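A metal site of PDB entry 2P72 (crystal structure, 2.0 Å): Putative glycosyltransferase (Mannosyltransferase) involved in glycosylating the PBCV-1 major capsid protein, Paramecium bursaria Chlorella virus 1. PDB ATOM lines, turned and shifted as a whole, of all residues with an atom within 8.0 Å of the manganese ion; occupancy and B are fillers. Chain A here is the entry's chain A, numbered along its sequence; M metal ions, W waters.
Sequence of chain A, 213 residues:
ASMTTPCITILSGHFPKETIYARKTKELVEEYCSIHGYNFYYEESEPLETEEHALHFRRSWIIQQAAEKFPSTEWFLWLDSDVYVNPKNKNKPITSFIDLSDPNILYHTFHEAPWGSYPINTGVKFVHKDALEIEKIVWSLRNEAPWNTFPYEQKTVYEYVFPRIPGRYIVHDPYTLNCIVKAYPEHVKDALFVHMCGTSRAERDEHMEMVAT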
ATOM      1  N   TYR A  21     -30.197 -15.657 -13.182  1.00  0.00           N
ATOM      2  CA  TYR A  21     -29.788 -15.101 -14.475  1.00  0.00           C
ATOM      3  C   TYR A  21     -28.474 -14.316 -14.370  1.00  0.00           C
ATOM      4  O   TYR A  21     -27.601 -14.490 -15.210  1.00  0.00           O
ATOM      5  CB  TYR A  21     -30.929 -14.269 -15.128  1.00  0.00           C
ATOM      6  CG  TYR A  21     -31.015 -12.809 -14.710  1.00  0.00           C
ATOM      7  CD1 TYR A  21     -30.077 -11.882 -15.168  1.00  0.00           C
ATOM      8  CD2 TYR A  21     -32.062 -12.351 -13.911  1.00  0.00           C
ATOM      9  CE1 TYR A  21     -30.149 -10.543 -14.786  1.00  0.00           C
ATOM     10  CE2 TYR A  21     -32.155 -11.005 -13.559  1.00  0.00           C
ATOM     11  CZ  TYR A  21     -31.184 -10.113 -13.982  1.00  0.00           C
ATOM     12  OH  TYR A  21     -31.237  -8.782 -13.631  1.00  0.00           O
ATOM     13  N   HIS A  56     -28.308   3.187 -11.402  1.00  0.00           N
ATOM     14  CA  HIS A  56     -27.949   3.312 -12.789  1.00  0.00           C
ATOM     15  C   HIS A  56     -26.581   3.978 -12.993  1.00  0.00           C
ATOM     16  O   HIS A  56     -25.847   3.619 -13.910  1.00  0.00           O
ATOM     17  CB  HIS A  56     -28.996   4.061 -13.608  1.00  0.00           C
ATOM     18  CG  HIS A  56     -28.688   4.055 -15.077  1.00  0.00           C
ATOM     19  ND1 HIS A  56     -27.719   4.849 -15.644  1.00  0.00           N
ATOM     20  CD2 HIS A  56     -29.169   3.278 -16.077  1.00  0.00           C
ATOM     21  CE1 HIS A  56     -27.640   4.602 -16.941  1.00  0.00           C
ATOM     22  NE2 HIS A  56     -28.507   3.635 -17.224  1.00  0.00           N
ATOM     23  N   ARG A  59     -22.378   2.153 -12.427  1.00  0.00           N
ATOM     24  CA  ARG A  59     -21.395   1.696 -13.392  1.00  0.00           C
ATOM     25  C   ARG A  59     -20.194   2.637 -13.506  1.00  0.00           C
ATOM     26  O   ARG A  59     -19.116   2.194 -13.890  1.00  0.00           O
ATOM     27  CB  ARG A  59     -22.042   1.471 -14.764  1.00  0.00           C
ATOM     28  CG  ARG A  59     -22.461   2.727 -15.524  1.00  0.00           C
ATOM     29  CD  ARG A  59     -23.365   2.345 -16.698  1.00  0.00           C
ATOM     30  NE  ARG A  59     -24.642   1.863 -16.173  1.00  0.00           N
ATOM     31  CZ  ARG A  59     -25.600   1.306 -16.906  1.00  0.00           C
ATOM     32  NH1 ARG A  59     -25.458   1.168 -18.208  1.00  0.00           N
ATOM     33  NH2 ARG A  59     -26.719   0.918 -16.312  1.00  0.00           N
ATOM     34  N   TRP A  78     -17.841  -1.991 -19.992  1.00  0.00           N
ATOM     35  CA  TRP A  78     -18.968  -2.238 -19.092  1.00  0.00           C
ATOM     36  C   TRP A  78     -20.017  -3.099 -19.802  1.00  0.00           C
ATOM     37  O   TRP A  78     -20.392  -2.796 -20.925  1.00  0.00           O
ATOM     38  CB  TRP A  78     -19.639  -0.930 -18.666  1.00  0.00           C
ATOM     39  CG  TRP A  78     -20.924  -1.187 -17.930  1.00  0.00           C
ATOM     40  CD1 TRP A  78     -22.194  -1.155 -18.463  1.00  0.00           C
ATOM     41  CD2 TRP A  78     -21.061  -1.586 -16.558  1.00  0.00           C
ATOM     42  NE1 TRP A  78     -23.123  -1.505 -17.472  1.00  0.00           N
ATOM     43  CE2 TRP A  78     -22.447  -1.756 -16.301  1.00  0.00           C
ATOM     44  CE3 TRP A  78     -20.154  -1.793 -15.519  1.00  0.00           C
ATOM     45  CZ2 TRP A  78     -22.947  -2.149 -15.029  1.00  0.00           C
ATOM     46  CZ3 TRP A  78     -20.663  -2.172 -14.225  1.00  0.00           C
ATOM     47  CH2 TRP A  78     -22.033  -2.338 -14.007  1.00  0.00           C
ATOM     48  N   LEU A  79     -20.477  -4.157 -19.131  1.00  0.00           N
ATOM     49  CA  LEU A  79     -21.634  -4.961 -19.579  1.00  0.00           C
ATOM     50  C   LEU A  79     -22.649  -5.006 -18.466  1.00  0.00           C
ATOM     51  O   LEU A  79     -22.307  -5.318 -17.316  1.00  0.00           O
ATOM     52  CB  LEU A  79     -21.222  -6.407 -19.853  1.00  0.00           C
ATOM     53  CG  LEU A  79     -20.159  -6.683 -20.930  1.00  0.00           C
ATOM     54  CD1 LEU A  79     -19.915  -8.183 -21.102  1.00  0.00           C
ATOM     55  CD2 LEU A  79     -20.563  -6.061 -22.212  1.00  0.00           C
ATOM     56  N   ASP A  80     -23.905  -4.707 -18.767  1.00  0.00           N
ATOM     57  CA  ASP A  80     -24.976  -4.936 -17.768  1.00  0.00           C
ATOM     58  C   ASP A  80     -25.037  -6.404 -17.315  1.00  0.00           C
ATOM     59  O   ASP A  80     -24.565  -7.317 -18.016  1.00  0.00           O
ATOM     60  CB  ASP A  80     -26.349  -4.511 -18.325  1.00  0.00           C
ATOM     61  CG  ASP A  80     -26.543  -3.004 -18.364  1.00  0.00           C
ATOM     62  OD1 ASP A  80     -25.675  -2.270 -17.844  1.00  0.00           O
ATOM     63  OD2 ASP A  80     -27.541  -2.563 -18.969  1.00  0.00           O
ATOM     64  N   SER A  81     -25.651  -6.649 -16.162  1.00  0.00           N
ATOM     65  CA  SER A  81     -25.740  -7.997 -15.644  1.00  0.00           C
ATOM     66  C   SER A  81     -26.779  -8.807 -16.425  1.00  0.00           C
ATOM     67  O   SER A  81     -26.843 -10.039 -16.281  1.00  0.00           O
ATOM     68  CB  SER A  81     -26.042  -8.016 -14.139  1.00  0.00           C
ATOM     69  OG  SER A  81     -27.159  -7.208 -13.834  1.00  0.00           O
ATOM     70  N   ASP A  82     -27.569  -8.134 -17.267  1.00  0.00           N
ATOM     71  CA  ASP A  82     -28.546  -8.833 -18.124  1.00  0.00           C
ATOM     72  C   ASP A  82     -28.078  -8.980 -19.583  1.00  0.00           C
ATOM     73  O   ASP A  82     -28.864  -9.325 -20.477  1.00  0.00           O
ATOM     74  CB  ASP A  82     -29.938  -8.182 -18.020  1.00  0.00           C
ATOM     75  CG  ASP A  82     -29.992  -6.772 -18.573  1.00  0.00           C
ATOM     76  OD1 ASP A  82     -31.000  -6.395 -19.213  1.00  0.00           O
ATOM     77  OD2 ASP A  82     -29.055  -6.013 -18.371  1.00  0.00           O
ATOM     78  N   VAL A  83     -26.778  -8.738 -19.779  1.00  0.00           N
ATOM     79  CA  VAL A  83     -26.080  -8.948 -21.045  1.00  0.00           C
ATOM     80  C   VAL A  83     -25.222 -10.200 -20.886  1.00  0.00           C
ATOM     81  O   VAL A  83     -24.497 -10.327 -19.891  1.00  0.00           O
ATOM     82  CB  VAL A  83     -25.136  -7.733 -21.350  1.00  0.00           C
ATOM     83  CG1 VAL A  83     -24.207  -8.015 -22.547  1.00  0.00           C
ATOM     84  CG2 VAL A  83     -25.950  -6.459 -21.574  1.00  0.00           C
ATOM     85  N   ASN A 121     -27.625   3.151 -26.022  1.00  0.00           N
ATOM     86  CA  ASN A 121     -27.906   2.221 -24.924  1.00  0.00           C
ATOM     87  C   ASN A 121     -26.561   1.878 -24.279  1.00  0.00           C
ATOM     88  O   ASN A 121     -25.689   1.265 -24.926  1.00  0.00           O
ATOM     89  CB  ASN A 121     -28.625   0.978 -25.463  1.00  0.00           C
ATOM     90  CG  ASN A 121     -29.028   0.046 -24.362  1.00  0.00           C
ATOM     91  OD1 ASN A 121     -28.187  -0.497 -23.664  1.00  0.00           O
ATOM     92  ND2 ASN A 121     -30.325  -0.141 -24.205  1.00  0.00           N
ATOM     93  N   THR A 122     -26.346   2.330 -23.046  1.00  0.00           N
ATOM     94  CA  THR A 122     -25.045   2.111 -22.397  1.00  0.00           C
ATOM     95  C   THR A 122     -24.939   0.788 -21.639  1.00  0.00           C
ATOM     96  O   THR A 122     -24.033   0.631 -20.814  1.00  0.00           O
ATOM     97  CB  THR A 122     -24.620   3.307 -21.445  1.00  0.00           C
ATOM     98  OG1 THR A 122     -25.680   3.604 -20.528  1.00  0.00           O
ATOM     99  CG2 THR A 122     -24.303   4.554 -22.228  1.00  0.00           C
ATOM    100  N   GLY A 123     -25.872  -0.138 -21.896  1.00  0.00           N
ATOM    101  CA  GLY A 123     -25.788  -1.526 -21.388  1.00  0.00           C
ATOM    102  C   GLY A 123     -24.488  -2.245 -21.777  1.00  0.00           C
ATOM    103  O   GLY A 123     -24.034  -3.156 -21.096  1.00  0.00           O
ATOM    104  N   VAL A 124     -23.909  -1.793 -22.868  1.00  0.00           N
ATOM    105  CA  VAL A 124     -22.592  -2.216 -23.358  1.00  0.00           C
ATOM    106  C   VAL A 124     -21.885  -0.922 -23.720  1.00  0.00           C
ATOM    107  O   VAL A 124     -22.362  -0.162 -24.547  1.00  0.00           O
ATOM    108  CB  VAL A 124     -22.718  -3.135 -24.624  1.00  0.00           C
ATOM    109  CG1 VAL A 124     -21.319  -3.561 -25.141  1.00  0.00           C
ATOM    110  CG2 VAL A 124     -23.565  -4.336 -24.270  1.00  0.00           C
ATOM    111  N   GLN A 154     -26.828   7.150 -18.834  1.00  0.00           N
ATOM    112  CA  GLN A 154     -26.918   7.066 -20.289  1.00  0.00           C
ATOM    113  C   GLN A 154     -27.163   8.456 -20.908  1.00  0.00           C
ATOM    114  O   GLN A 154     -26.564   8.793 -21.931  1.00  0.00           O
ATOM    115  CB  GLN A 154     -28.003   6.044 -20.647  1.00  0.00           C
ATOM    116  CG  GLN A 154     -28.328   5.816 -22.095  1.00  0.00           C
ATOM    117  CD  GLN A 154     -29.295   4.651 -22.231  1.00  0.00           C
ATOM    118  OE1 GLN A 154     -28.888   3.487 -22.118  1.00  0.00           O
ATOM    119  NE2 GLN A 154     -30.579   4.962 -22.378  1.00  0.00           N
ATOM    120  N   ASN A 178     -24.580  -5.103 -28.931  1.00  0.00           N
ATOM    121  CA  ASN A 178     -25.577  -4.730 -27.912  1.00  0.00           C
ATOM    122  C   ASN A 178     -26.957  -5.138 -28.401  1.00  0.00           C
ATOM    123  O   ASN A 178     -27.844  -4.304 -28.610  1.00  0.00           O
ATOM    124  CB  ASN A 178     -25.481  -3.221 -27.536  1.00  0.00           C
ATOM    125  CG  ASN A 178     -26.297  -2.863 -26.285  1.00  0.00           C
ATOM    126  OD1 ASN A 178     -27.102  -3.680 -25.786  1.00  0.00           O
ATOM    127  ND2 ASN A 178     -26.114  -1.639 -25.790  1.00  0.00           N
ATOM    128  N   ILE A 180     -30.264  -6.261 -28.266  1.00  0.00           N
ATOM    129  CA  ILE A 180     -31.450  -6.379 -27.424  1.00  0.00           C
ATOM    130  C   ILE A 180     -32.343  -7.503 -27.956  1.00  0.00           C
ATOM    131  O   ILE A 180     -32.801  -7.479 -29.112  1.00  0.00           O
ATOM    132  CB  ILE A 180     -32.213  -5.013 -27.298  1.00  0.00           C
ATOM    133  CG1 ILE A 180     -31.267  -3.980 -26.628  1.00  0.00           C
ATOM    134  CG2 ILE A 180     -33.591  -5.174 -26.587  1.00  0.00           C
ATOM    135  CD1 ILE A 180     -31.683  -2.531 -26.854  1.00  0.00           C
ATOM    136  N   VAL A 194     -25.531 -10.316 -26.066  1.00  0.00           N
ATOM    137  CA  VAL A 194     -26.995 -10.332 -26.108  1.00  0.00           C
ATOM    138  C   VAL A 194     -27.528  -9.638 -24.863  1.00  0.00           C
ATOM    139  O   VAL A 194     -27.131  -9.966 -23.734  1.00  0.00           O
ATOM    140  CB  VAL A 194     -27.561 -11.794 -26.285  1.00  0.00           C
ATOM    141  CG1 VAL A 194     -29.067 -11.812 -26.483  1.00  0.00           C
ATOM    142  CG2 VAL A 194     -26.909 -12.497 -27.484  1.00  0.00           C
ATOM    143  N   HIS A 195     -28.401  -8.665 -25.062  1.00  0.00           N
ATOM    144  CA  HIS A 195     -28.873  -7.799 -23.992  1.00  0.00           C
ATOM    145  C   HIS A 195     -30.316  -8.143 -23.724  1.00  0.00           C
ATOM    146  O   HIS A 195     -31.167  -7.996 -24.598  1.00  0.00           O
ATOM    147  CB  HIS A 195     -28.782  -6.330 -24.433  1.00  0.00           C
ATOM    148  CG  HIS A 195     -28.916  -5.349 -23.311  1.00  0.00           C
ATOM    149  ND1 HIS A 195     -28.483  -4.040 -23.419  1.00  0.00           N
ATOM    150  CD2 HIS A 195     -29.417  -5.482 -22.056  1.00  0.00           C
ATOM    151  CE1 HIS A 195     -28.696  -3.414 -22.273  1.00  0.00           C
ATOM    152  NE2 HIS A 195     -29.264  -4.262 -21.430  1.00  0.00           N
ATOM    153  N   MET A 196     -30.597  -8.611 -22.518  1.00  0.00           N
ATOM    154  CA  MET A 196     -31.959  -8.969 -22.156  1.00  0.00           C
ATOM    155  C   MET A 196     -32.655  -7.758 -21.568  1.00  0.00           C
ATOM    156  O   MET A 196     -33.196  -7.826 -20.465  1.00  0.00           O
ATOM    157  CB  MET A 196     -31.972 -10.141 -21.187  1.00  0.00           C
ATOM    158  CG  MET A 196     -31.279 -11.407 -21.664  1.00  0.00           C
ATOM    159  SD  MET A 196     -31.408 -12.710 -20.412  1.00  0.00           S
ATOM    160  CE  MET A 196     -30.272 -12.138 -19.134  1.00  0.00           C
ATOM    161  N   CYS A 197     -32.584  -6.647 -22.300  1.00  0.00           N
ATOM    162  CA  CYS A 197     -33.261  -5.390 -21.978  1.00  0.00           C
ATOM    163  C   CYS A 197     -34.767  -5.457 -22.329  1.00  0.00           C
ATOM    164  O   CYS A 197     -35.159  -5.761 -23.480  1.00  0.00           O
ATOM    165  CB  CYS A 197     -32.591  -4.251 -22.744  1.00  0.00           C
ATOM    166  SG  CYS A 197     -33.172  -2.573 -22.388  1.00  0.00           S
ATOM    167  N   GLY A 198     -35.595  -5.131 -21.353  1.00  0.00           N
ATOM    168  CA  GLY A 198     -37.049  -5.173 -21.533  1.00  0.00           C
ATOM    169  C   GLY A 198     -37.690  -6.128 -20.542  1.00  0.00           C
ATOM    170  O   GLY A 198     -37.179  -6.310 -19.427  1.00  0.00           O
ATOM    171  N   ARG A 204     -35.792 -13.434 -17.681  1.00  0.00           N
ATOM    172  CA  ARG A 204     -34.333 -13.540 -17.839  1.00  0.00           C
ATOM    173  C   ARG A 204     -33.769 -14.888 -17.419  1.00  0.00           C
ATOM    174  O   ARG A 204     -32.951 -15.480 -18.136  1.00  0.00           O
ATOM    175  CB  ARG A 204     -33.642 -12.405 -17.090  1.00  0.00           C
ATOM    176  CG  ARG A 204     -34.022 -11.043 -17.599  1.00  0.00           C
ATOM    177  CD  ARG A 204     -33.263  -9.945 -16.905  1.00  0.00           C
ATOM    178  NE  ARG A 204     -33.483  -8.686 -17.602  1.00  0.00           N
ATOM    179  CZ  ARG A 204     -33.271  -7.487 -17.080  1.00  0.00           C
ATOM    180  NH1 ARG A 204     -32.847  -7.365 -15.833  1.00  0.00           N
ATOM    181  NH2 ARG A 204     -33.506  -6.406 -17.815  1.00  0.00           N
HETATM  182 MN    MN M   1     -29.487  -3.896 -19.214  1.00  0.00          MN
HETATM  183  O   HOH W   1     -29.771  -3.499 -17.200  1.00  0.00           O
HETATM  184  O   HOH W   2     -30.665  -2.328 -19.713  1.00  0.00           O
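ND1 of His 195 is in hydrogen-bond range of OD1 of Asn 178 (2.8 Å).
The backbone NH (N) of Cys 197 lies within hydrogen-bond range of the side-chain carboxylate (OD1) of Asp 82 (3.5 Å).
The side-chain carboxylate of Asp 82 is in salt-bridge range of the guanidinium group of Arg 204.
The backbone NH (N) of Met 196 sits at hydrogen-bond distance from the backbone carbonyl oxygen (O) of Asp 82, at 2.8 Å.
N of Asp 80 is in hydrogen-bond range of O of Gly 123, 2.8 Å away.
The guanidinium group of Arg 59 lies within salt-bridge range of the side-chain carboxylate of Asp 80 (3.5 Å).
OD1 of Asp 80 is in hydrogen-bond range of NE1 of Trp 78 (2.7 Å).
Water W2 binds the manganese ion (2.0 Å).
The manganese ion is bound by water W1 (2.1 Å).
A ring nitrogen (NE2) of His 195 is bound to the manganese ion, at 2.3 Å.
OD2 of Asp 82 binds the manganese ion (2.3 Å).
OD2 of Asp 80 binds the manganese ion.
Slightly farther from the manganese ion lies the side-chain carboxylate (OD1) of Asp 82 (2.9 Å).
Within 4 Å of the manganese ion: Asp 80, Asp 82 and His 195.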
